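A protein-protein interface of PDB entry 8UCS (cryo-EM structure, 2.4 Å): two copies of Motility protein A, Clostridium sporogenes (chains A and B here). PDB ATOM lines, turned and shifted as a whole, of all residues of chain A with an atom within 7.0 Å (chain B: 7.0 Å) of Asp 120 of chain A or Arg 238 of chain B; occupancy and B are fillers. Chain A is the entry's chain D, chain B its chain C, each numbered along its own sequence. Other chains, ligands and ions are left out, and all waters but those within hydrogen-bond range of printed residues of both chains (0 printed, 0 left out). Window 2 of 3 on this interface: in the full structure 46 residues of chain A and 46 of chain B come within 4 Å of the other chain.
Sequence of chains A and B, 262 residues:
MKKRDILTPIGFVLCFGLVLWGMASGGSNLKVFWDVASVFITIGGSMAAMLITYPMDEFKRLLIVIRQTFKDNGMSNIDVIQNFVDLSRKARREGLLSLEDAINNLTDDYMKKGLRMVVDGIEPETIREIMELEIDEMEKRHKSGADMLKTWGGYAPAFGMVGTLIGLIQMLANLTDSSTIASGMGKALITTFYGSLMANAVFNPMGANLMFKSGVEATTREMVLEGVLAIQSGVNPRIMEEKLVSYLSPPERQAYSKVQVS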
ATOM      1  N   LEU A  96     -11.564  12.425  -1.598  1.00  0.00           N
ATOM      2  CA  LEU A  96     -12.131  13.384  -0.655  1.00  0.00           C
ATOM      3  C   LEU A  96     -11.586  14.785  -0.890  1.00  0.00           C
ATOM      4  O   LEU A  96     -12.300  15.771  -0.680  1.00  0.00           O
ATOM      5  CB  LEU A  96     -11.854  12.942   0.782  1.00  0.00           C
ATOM      6  CG  LEU A  96     -12.827  11.923   1.375  1.00  0.00           C
ATOM      7  CD1 LEU A  96     -12.493  11.648   2.830  1.00  0.00           C
ATOM      8  CD2 LEU A  96     -14.258  12.409   1.233  1.00  0.00           C
ATOM      9  N   LEU A  97     -10.333  14.893  -1.325  1.00  0.00           N
ATOM     10  CA  LEU A  97      -9.769  16.187  -1.669  1.00  0.00           C
ATOM     11  C   LEU A  97     -10.364  16.682  -2.986  1.00  0.00           C
ATOM     12  O   LEU A  97     -11.257  16.060  -3.571  1.00  0.00           O
ATOM     13  CB  LEU A  97      -8.248  16.102  -1.751  1.00  0.00           C
ATOM     14  CG  LEU A  97      -7.494  16.776  -0.604  1.00  0.00           C
ATOM     15  CD1 LEU A  97      -7.692  16.012   0.699  1.00  0.00           C
ATOM     16  CD2 LEU A  97      -6.022  16.912  -0.939  1.00  0.00           C
ATOM     17  N   GLU A 100     -12.298  21.156  -1.928  1.00  0.00           N
ATOM     18  CA  GLU A 100     -12.110  22.408  -1.204  1.00  0.00           C
ATOM     19  C   GLU A 100     -12.815  23.563  -1.901  1.00  0.00           C
ATOM     20  O   GLU A 100     -13.449  24.397  -1.245  1.00  0.00           O
ATOM     21  CB  GLU A 100     -10.617  22.704  -1.054  1.00  0.00           C
ATOM     22  CG  GLU A 100     -10.271  23.562   0.152  1.00  0.00           C
ATOM     23  CD  GLU A 100      -9.799  22.739   1.335  1.00  0.00           C
ATOM     24  OE1 GLU A 100     -10.656  22.258   2.106  1.00  0.00           O
ATOM     25  OE2 GLU A 100      -8.572  22.574   1.493  1.00  0.00           O
ATOM     26  N   LYS A 113     -18.341  23.449   8.055  1.00  0.00           N
ATOM     27  CA  LYS A 113     -17.558  23.030   9.212  1.00  0.00           C
ATOM     28  C   LYS A 113     -17.361  21.519   9.225  1.00  0.00           C
ATOM     29  O   LYS A 113     -16.247  21.028   9.444  1.00  0.00           O
ATOM     30  CB  LYS A 113     -18.238  23.500  10.496  1.00  0.00           C
ATOM     31  CG  LYS A 113     -17.406  23.306  11.749  1.00  0.00           C
ATOM     32  CD  LYS A 113     -18.280  22.976  12.946  1.00  0.00           C
ATOM     33  CE  LYS A 113     -17.466  22.947  14.227  1.00  0.00           C
ATOM     34  NZ  LYS A 113     -17.783  24.093  15.124  1.00  0.00           N
ATOM     35  N   LEU A 115     -17.702  19.388   6.623  1.00  0.00           N
ATOM     36  CA  LEU A 115     -16.995  18.917   5.437  1.00  0.00           C
ATOM     37  C   LEU A 115     -15.513  19.259   5.490  1.00  0.00           C
ATOM     38  O   LEU A 115     -14.688  18.503   4.967  1.00  0.00           O
ATOM     39  CB  LEU A 115     -17.633  19.501   4.178  1.00  0.00           C
ATOM     40  CG  LEU A 115     -18.961  18.867   3.760  1.00  0.00           C
ATOM     41  CD1 LEU A 115     -19.572  19.617   2.591  1.00  0.00           C
ATOM     42  CD2 LEU A 115     -18.777  17.396   3.427  1.00  0.00           C
ATOM     43  N   ARG A 116     -15.156  20.392   6.100  1.00  0.00           N
ATOM     44  CA  ARG A 116     -13.747  20.733   6.253  1.00  0.00           C
ATOM     45  C   ARG A 116     -13.034  19.724   7.144  1.00  0.00           C
ATOM     46  O   ARG A 116     -11.892  19.338   6.869  1.00  0.00           O
ATOM     47  CB  ARG A 116     -13.605  22.146   6.814  1.00  0.00           C
ATOM     48  CG  ARG A 116     -13.427  23.209   5.745  1.00  0.00           C
ATOM     49  CD  ARG A 116     -13.782  24.589   6.264  1.00  0.00           C
ATOM     50  NE  ARG A 116     -13.728  25.590   5.206  1.00  0.00           N
ATOM     51  CZ  ARG A 116     -14.585  26.595   5.078  1.00  0.00           C
ATOM     52  NH1 ARG A 116     -15.579  26.767   5.933  1.00  0.00           N
ATOM     53  NH2 ARG A 116     -14.440  27.446   4.067  1.00  0.00           N
ATOM     54  N   MET A 117     -13.690  19.290   8.222  1.00  0.00           N
ATOM     55  CA  MET A 117     -13.127  18.233   9.052  1.00  0.00           C
ATOM     56  C   MET A 117     -13.025  16.921   8.286  1.00  0.00           C
ATOM     57  O   MET A 117     -12.091  16.143   8.509  1.00  0.00           O
ATOM     58  CB  MET A 117     -13.973  18.053  10.311  1.00  0.00           C
ATOM     59  CG  MET A 117     -14.020  19.283  11.202  1.00  0.00           C
ATOM     60  SD  MET A 117     -14.819  18.975  12.787  1.00  0.00           S
ATOM     61  CE  MET A 117     -16.483  18.582  12.255  1.00  0.00           C
ATOM     62  N   VAL A 118     -13.977  16.656   7.389  1.00  0.00           N
ATOM     63  CA  VAL A 118     -13.928  15.446   6.573  1.00  0.00           C
ATOM     64  C   VAL A 118     -12.726  15.484   5.638  1.00  0.00           C
ATOM     65  O   VAL A 118     -11.992  14.497   5.499  1.00  0.00           O
ATOM     66  CB  VAL A 118     -15.246  15.281   5.792  1.00  0.00           C
ATOM     67  CG1 VAL A 118     -15.041  14.406   4.562  1.00  0.00           C
ATOM     68  CG2 VAL A 118     -16.321  14.708   6.690  1.00  0.00           C
ATOM     69  N   VAL A 119     -12.503  16.626   4.988  1.00  0.00           N
ATOM     70  CA  VAL A 119     -11.396  16.749   4.045  1.00  0.00           C
ATOM     71  C   VAL A 119     -10.059  16.669   4.773  1.00  0.00           C
ATOM     72  O   VAL A 119      -9.103  16.057   4.279  1.00  0.00           O
ATOM     73  CB  VAL A 119     -11.535  18.054   3.238  1.00  0.00           C
ATOM     74  CG1 VAL A 119     -10.200  18.474   2.645  1.00  0.00           C
ATOM     75  CG2 VAL A 119     -12.578  17.886   2.144  1.00  0.00           C
ATOM     76  N   ASP A 120      -9.974  17.268   5.964  1.00  0.00           N
ATOM     77  CA  ASP A 120      -8.724  17.250   6.717  1.00  0.00           C
ATOM     78  C   ASP A 120      -8.346  15.842   7.157  1.00  0.00           C
ATOM     79  O   ASP A 120      -7.156  15.534   7.287  1.00  0.00           O
ATOM     80  CB  ASP A 120      -8.830  18.169   7.931  1.00  0.00           C
ATOM     81  CG  ASP A 120      -8.923  19.626   7.547  1.00  0.00           C
ATOM     82  OD1 ASP A 120      -8.732  19.941   6.355  1.00  0.00           O
ATOM     83  OD2 ASP A 120      -9.190  20.456   8.437  1.00  0.00           O
ATOM     84  N   GLY A 121      -9.330  14.980   7.393  1.00  0.00           N
ATOM     85  CA  GLY A 121      -9.051  13.624   7.816  1.00  0.00           C
ATOM     86  C   GLY A 121      -9.278  13.393   9.295  1.00  0.00           C
ATOM     87  O   GLY A 121      -8.476  12.729   9.958  1.00  0.00           O
ATOM     88  N   ILE A 122     -10.365  13.938   9.820  1.00  0.00           N
ATOM     89  CA  ILE A 122     -10.739  13.761  11.217  1.00  0.00           C
ATOM     90  C   ILE A 122     -11.626  12.532  11.331  1.00  0.00           C
ATOM     91  O   ILE A 122     -12.459  12.267  10.456  1.00  0.00           O
ATOM     92  CB  ILE A 122     -11.442  15.024  11.752  1.00  0.00           C
ATOM     93  CG1 ILE A 122     -10.517  16.235  11.610  1.00  0.00           C
ATOM     94  CG2 ILE A 122     -11.878  14.835  13.199  1.00  0.00           C
ATOM     95  CD1 ILE A 122     -10.792  17.340  12.598  1.00  0.00           C
ATOM     96  N   ILE A 130     -18.566  16.609  17.615  1.00  0.00           N
ATOM     97  CA  ILE A 130     -18.454  18.053  17.439  1.00  0.00           C
ATOM     98  C   ILE A 130     -19.705  18.608  16.771  1.00  0.00           C
ATOM     99  O   ILE A 130     -20.239  19.644  17.183  1.00  0.00           O
ATOM    100  CB  ILE A 130     -17.184  18.395  16.639  1.00  0.00           C
ATOM    101  CG1 ILE A 130     -15.939  18.211  17.507  1.00  0.00           C
ATOM    102  CG2 ILE A 130     -17.249  19.814  16.100  1.00  0.00           C
ATOM    103  CD1 ILE A 130     -14.646  18.393  16.756  1.00  0.00           C
ATOM    104  N   VAL B  85      -6.851  27.082  24.208  1.00  0.00           N
ATOM    105  CA  VAL B  85      -6.018  26.840  23.034  1.00  0.00           C
ATOM    106  C   VAL B  85      -4.550  27.075  23.364  1.00  0.00           C
ATOM    107  O   VAL B  85      -3.678  26.291  22.972  1.00  0.00           O
ATOM    108  CB  VAL B  85      -6.490  27.714  21.857  1.00  0.00           C
ATOM    109  CG1 VAL B  85      -5.399  27.831  20.803  1.00  0.00           C
ATOM    110  CG2 VAL B  85      -7.758  27.141  21.249  1.00  0.00           C
ATOM    111  N   SER B  88      -3.377  24.208  25.625  1.00  0.00           N
ATOM    112  CA  SER B  88      -3.220  22.957  24.889  1.00  0.00           C
ATOM    113  C   SER B  88      -1.967  22.977  24.023  1.00  0.00           C
ATOM    114  O   SER B  88      -1.284  21.956  23.888  1.00  0.00           O
ATOM    115  CB  SER B  88      -4.459  22.687  24.038  1.00  0.00           C
ATOM    116  OG  SER B  88      -4.414  23.410  22.822  1.00  0.00           O
ATOM    117  N   ARG B  89      -1.655  24.126  23.420  1.00  0.00           N
ATOM    118  CA  ARG B  89      -0.424  24.241  22.646  1.00  0.00           C
ATOM    119  C   ARG B  89       0.803  24.120  23.539  1.00  0.00           C
ATOM    120  O   ARG B  89       1.784  23.463  23.172  1.00  0.00           O
ATOM    121  CB  ARG B  89      -0.404  25.566  21.885  1.00  0.00           C
ATOM    122  CG  ARG B  89      -1.317  25.596  20.674  1.00  0.00           C
ATOM    123  CD  ARG B  89      -0.703  26.394  19.536  1.00  0.00           C
ATOM    124  NE  ARG B  89      -1.724  26.936  18.647  1.00  0.00           N
ATOM    125  CZ  ARG B  89      -2.372  28.073  18.860  1.00  0.00           C
ATOM    126  NH1 ARG B  89      -2.125  28.822  19.921  1.00  0.00           N
ATOM    127  NH2 ARG B  89      -3.291  28.469  17.984  1.00  0.00           N
ATOM    128  N   VAL B 235      -5.613  16.195  23.049  1.00  0.00           N
ATOM    129  CA  VAL B 235      -6.196  16.414  21.732  1.00  0.00           C
ATOM    130  C   VAL B 235      -5.447  17.531  21.014  1.00  0.00           C
ATOM    131  O   VAL B 235      -4.727  18.330  21.620  1.00  0.00           O
ATOM    132  CB  VAL B 235      -7.701  16.725  21.830  1.00  0.00           C
ATOM    133  CG1 VAL B 235      -8.370  15.798  22.828  1.00  0.00           C
ATOM    134  CG2 VAL B 235      -7.923  18.178  22.207  1.00  0.00           C
ATOM    135  N   ASN B 236      -5.614  17.576  19.698  1.00  0.00           N
ATOM    136  CA  ASN B 236      -4.975  18.611  18.901  1.00  0.00           C
ATOM    137  C   ASN B 236      -5.566  19.978  19.243  1.00  0.00           C
ATOM    138  O   ASN B 236      -6.773  20.090  19.478  1.00  0.00           O
ATOM    139  CB  ASN B 236      -5.154  18.321  17.412  1.00  0.00           C
ATOM    140  CG  ASN B 236      -4.147  19.052  16.551  1.00  0.00           C
ATOM    141  OD1 ASN B 236      -2.949  19.044  16.835  1.00  0.00           O
ATOM    142  ND2 ASN B 236      -4.627  19.689  15.490  1.00  0.00           N
ATOM    143  N   PRO B 237      -4.743  21.028  19.294  1.00  0.00           N
ATOM    144  CA  PRO B 237      -5.291  22.368  19.558  1.00  0.00           C
ATOM    145  C   PRO B 237      -6.329  22.813  18.544  1.00  0.00           C
ATOM    146  O   PRO B 237      -7.245  23.562  18.901  1.00  0.00           O
ATOM    147  CB  PRO B 237      -4.046  23.264  19.526  1.00  0.00           C
ATOM    148  CG  PRO B 237      -2.930  22.357  19.895  1.00  0.00           C
ATOM    149  CD  PRO B 237      -3.272  21.022  19.305  1.00  0.00           C
ATOM    150  N   ARG B 238      -6.214  22.385  17.286  1.00  0.00           N
ATOM    151  CA  ARG B 238      -7.246  22.715  16.309  1.00  0.00           C
ATOM    152  C   ARG B 238      -8.537  21.962  16.604  1.00  0.00           C
ATOM    153  O   ARG B 238      -9.631  22.529  16.508  1.00  0.00           O
ATOM    154  CB  ARG B 238      -6.763  22.403  14.892  1.00  0.00           C
ATOM    155  CG  ARG B 238      -7.854  22.548  13.845  1.00  0.00           C
ATOM    156  CD  ARG B 238      -8.273  21.213  13.256  1.00  0.00           C
ATOM    157  NE  ARG B 238      -8.762  21.357  11.890  1.00  0.00           N
ATOM    158  CZ  ARG B 238      -9.987  21.034  11.499  1.00  0.00           C
ATOM    159  NH1 ARG B 238     -10.887  20.580  12.354  1.00  0.00           N
ATOM    160  NH2 ARG B 238     -10.322  21.184  10.221  1.00  0.00           N
ATOM    161  N   ILE B 239      -8.427  20.680  16.961  1.00  0.00           N
ATOM    162  CA  ILE B 239      -9.609  19.901  17.316  1.00  0.00           C
ATOM    163  C   ILE B 239     -10.239  20.447  18.590  1.00  0.00           C
ATOM    164  O   ILE B 239     -11.468  20.518  18.711  1.00  0.00           O
ATOM    165  CB  ILE B 239      -9.243  18.412  17.453  1.00  0.00           C
ATOM    166  CG1 ILE B 239      -8.875  17.828  16.087  1.00  0.00           C
ATOM    167  CG2 ILE B 239     -10.387  17.634  18.088  1.00  0.00           C
ATOM    168  CD1 ILE B 239      -8.971  16.318  16.014  1.00  0.00           C
ATOM    169  N   MET B 240      -9.411  20.840  19.560  1.00  0.00           N
ATOM    170  CA  MET B 240      -9.928  21.459  20.775  1.00  0.00           C
ATOM    171  C   MET B 240     -10.677  22.745  20.454  1.00  0.00           C
ATOM    172  O   MET B 240     -11.777  22.981  20.966  1.00  0.00           O
ATOM    173  CB  MET B 240      -8.781  21.732  21.749  1.00  0.00           C
ATOM    174  CG  MET B 240      -9.033  22.901  22.687  1.00  0.00           C
ATOM    175  SD  MET B 240      -9.509  22.381  24.343  1.00  0.00           S
ATOM    176  CE  MET B 240      -7.905  22.255  25.123  1.00  0.00           C
ATOM    177  N   GLU B 241     -10.097  23.583  19.594  1.00  0.00           N
ATOM    178  CA  GLU B 241     -10.760  24.823  19.208  1.00  0.00           C
ATOM    179  C   GLU B 241     -12.050  24.544  18.449  1.00  0.00           C
ATOM    180  O   GLU B 241     -13.062  25.219  18.663  1.00  0.00           O
ATOM    181  CB  GLU B 241      -9.811  25.681  18.372  1.00  0.00           C
ATOM    182  CG  GLU B 241     -10.501  26.687  17.471  1.00  0.00           C
ATOM    183  CD  GLU B 241      -9.523  27.631  16.804  1.00  0.00           C
ATOM    184  OE1 GLU B 241      -8.301  27.455  16.996  1.00  0.00           O
ATOM    185  OE2 GLU B 241      -9.973  28.546  16.085  1.00  0.00           O
ATOM    186  N   GLU B 242     -12.038  23.542  17.565  1.00  0.00           N
ATOM    187  CA  GLU B 242     -13.235  23.213  16.798  1.00  0.00           C
ATOM    188  C   GLU B 242     -14.379  22.790  17.710  1.00  0.00           C
ATOM    189  O   GLU B 242     -15.527  23.201  17.512  1.00  0.00           O
ATOM    190  CB  GLU B 242     -12.920  22.110  15.789  1.00  0.00           C
ATOM    191  CG  GLU B 242     -13.902  22.021  14.638  1.00  0.00           C
ATOM    192  CD  GLU B 242     -13.444  22.800  13.423  1.00  0.00           C
ATOM    193  OE1 GLU B 242     -12.292  23.283  13.425  1.00  0.00           O
ATOM    194  OE2 GLU B 242     -14.234  22.928  12.464  1.00  0.00           O
ATOM    195  N   LYS B 243     -14.087  21.963  18.714  1.00  0.00           N
ATOM    196  CA  LYS B 243     -15.118  21.556  19.663  1.00  0.00           C
ATOM    197  C   LYS B 243     -15.503  22.706  20.585  1.00  0.00           C
ATOM    198  O   LYS B 243     -16.674  22.849  20.957  1.00  0.00           O
ATOM    199  CB  LYS B 243     -14.629  20.352  20.468  1.00  0.00           C
ATOM    200  CG  LYS B 243     -15.404  20.083  21.742  1.00  0.00           C
ATOM    201  CD  LYS B 243     -15.224  18.649  22.199  1.00  0.00           C
ATOM    202  CE  LYS B 243     -16.469  17.822  21.931  1.00  0.00           C
ATOM    203  NZ  LYS B 243     -16.515  16.603  22.782  1.00  0.00           N
ATOM    204  N   LEU B 244     -14.535  23.546  20.954  1.00  0.00           N
ATOM    205  CA  LEU B 244     -14.805  24.619  21.904  1.00  0.00           C
ATOM    206  C   LEU B 244     -15.649  25.727  21.282  1.00  0.00           C
ATOM    207  O   LEU B 244     -16.532  26.283  21.944  1.00  0.00           O
ATOM    208  CB  LEU B 244     -13.492  25.180  22.444  1.00  0.00           C
ATOM    209  CG  LEU B 244     -12.936  24.502  23.693  1.00  0.00           C
ATOM    210  CD1 LEU B 244     -11.779  25.301  24.254  1.00  0.00           C
ATOM    211  CD2 LEU B 244     -14.030  24.349  24.723  1.00  0.00           C
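The side-chain amino group (NZ) of Lys 113 of chain A sits at hydrogen-bond distance from the backbone carbonyl oxygen (O) of Glu 242 of chain B, at 3.4 Å. The guanidinium group (NE) of Arg 238 of chain B is in salt-bridge range of the side-chain carboxylate (OD2) of Asp 120 of chain A (3.6 Å).
The guanidinium group (NH1) of Arg 238 of chain B is in salt-bridge range of the side-chain carboxylate (OE1) of Glu 242 of chain B (3.2 Å). N of Ile 122 of chain A sits at hydrogen-bond distance from O of Met 117 of chain A, at 3.1 Å.
Arg 238 of chain B touches Met 117 of chain A (NH1 to CG, 3.6 Å). CG of Glu 242 of chain B touches SD of Met 117 of chain A, at 3.7 Å. CD1 of Ile 122 of chain A touches NH1 of Arg 238 of chain B, 3.3 Å away. CB of Lys 243 of chain B touches CG1 of Ile 130 of chain A, 3.9 Å away.
Printed residues of chain B within 4 Å of Lys 113 of chain A: Glu 242 (3.3 Å). Of chain B, only Arg 238 comes within 4 Å of Asp 120 of chain A. Of the printed residues of chain B, Ile 130 of chain A touches Lys 243 (3.9 Å). Arg 238 of chain B touches just these residues of chain A: Met 117, Asp 120 and Ile 122. The nearest residue of chain B that does not touch Asp 120 of chain A is Glu 242 of chain B (6.5 Å). The nearest printed residue of chain A that does not touch Glu 242 of chain B is Ile 130 of chain A (4.1 Å).
Of the 13 printed residues of chain B, 3 touch a printed residue of chain A. Printed residues of chain B that touch a printed residue of chain A: Arg 238, Glu 242 and Lys 243. Of the 13 printed residues of chain A, 5 touch a printed residue of chain B. Hydrophobic or aromatic side chains of chain A within 4 Å of the printed part of chain B: Met 117, Ile 122 and Ile 130. Among the printed residues, 6 pairs touch across the chains.
No position is printed for both chains.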
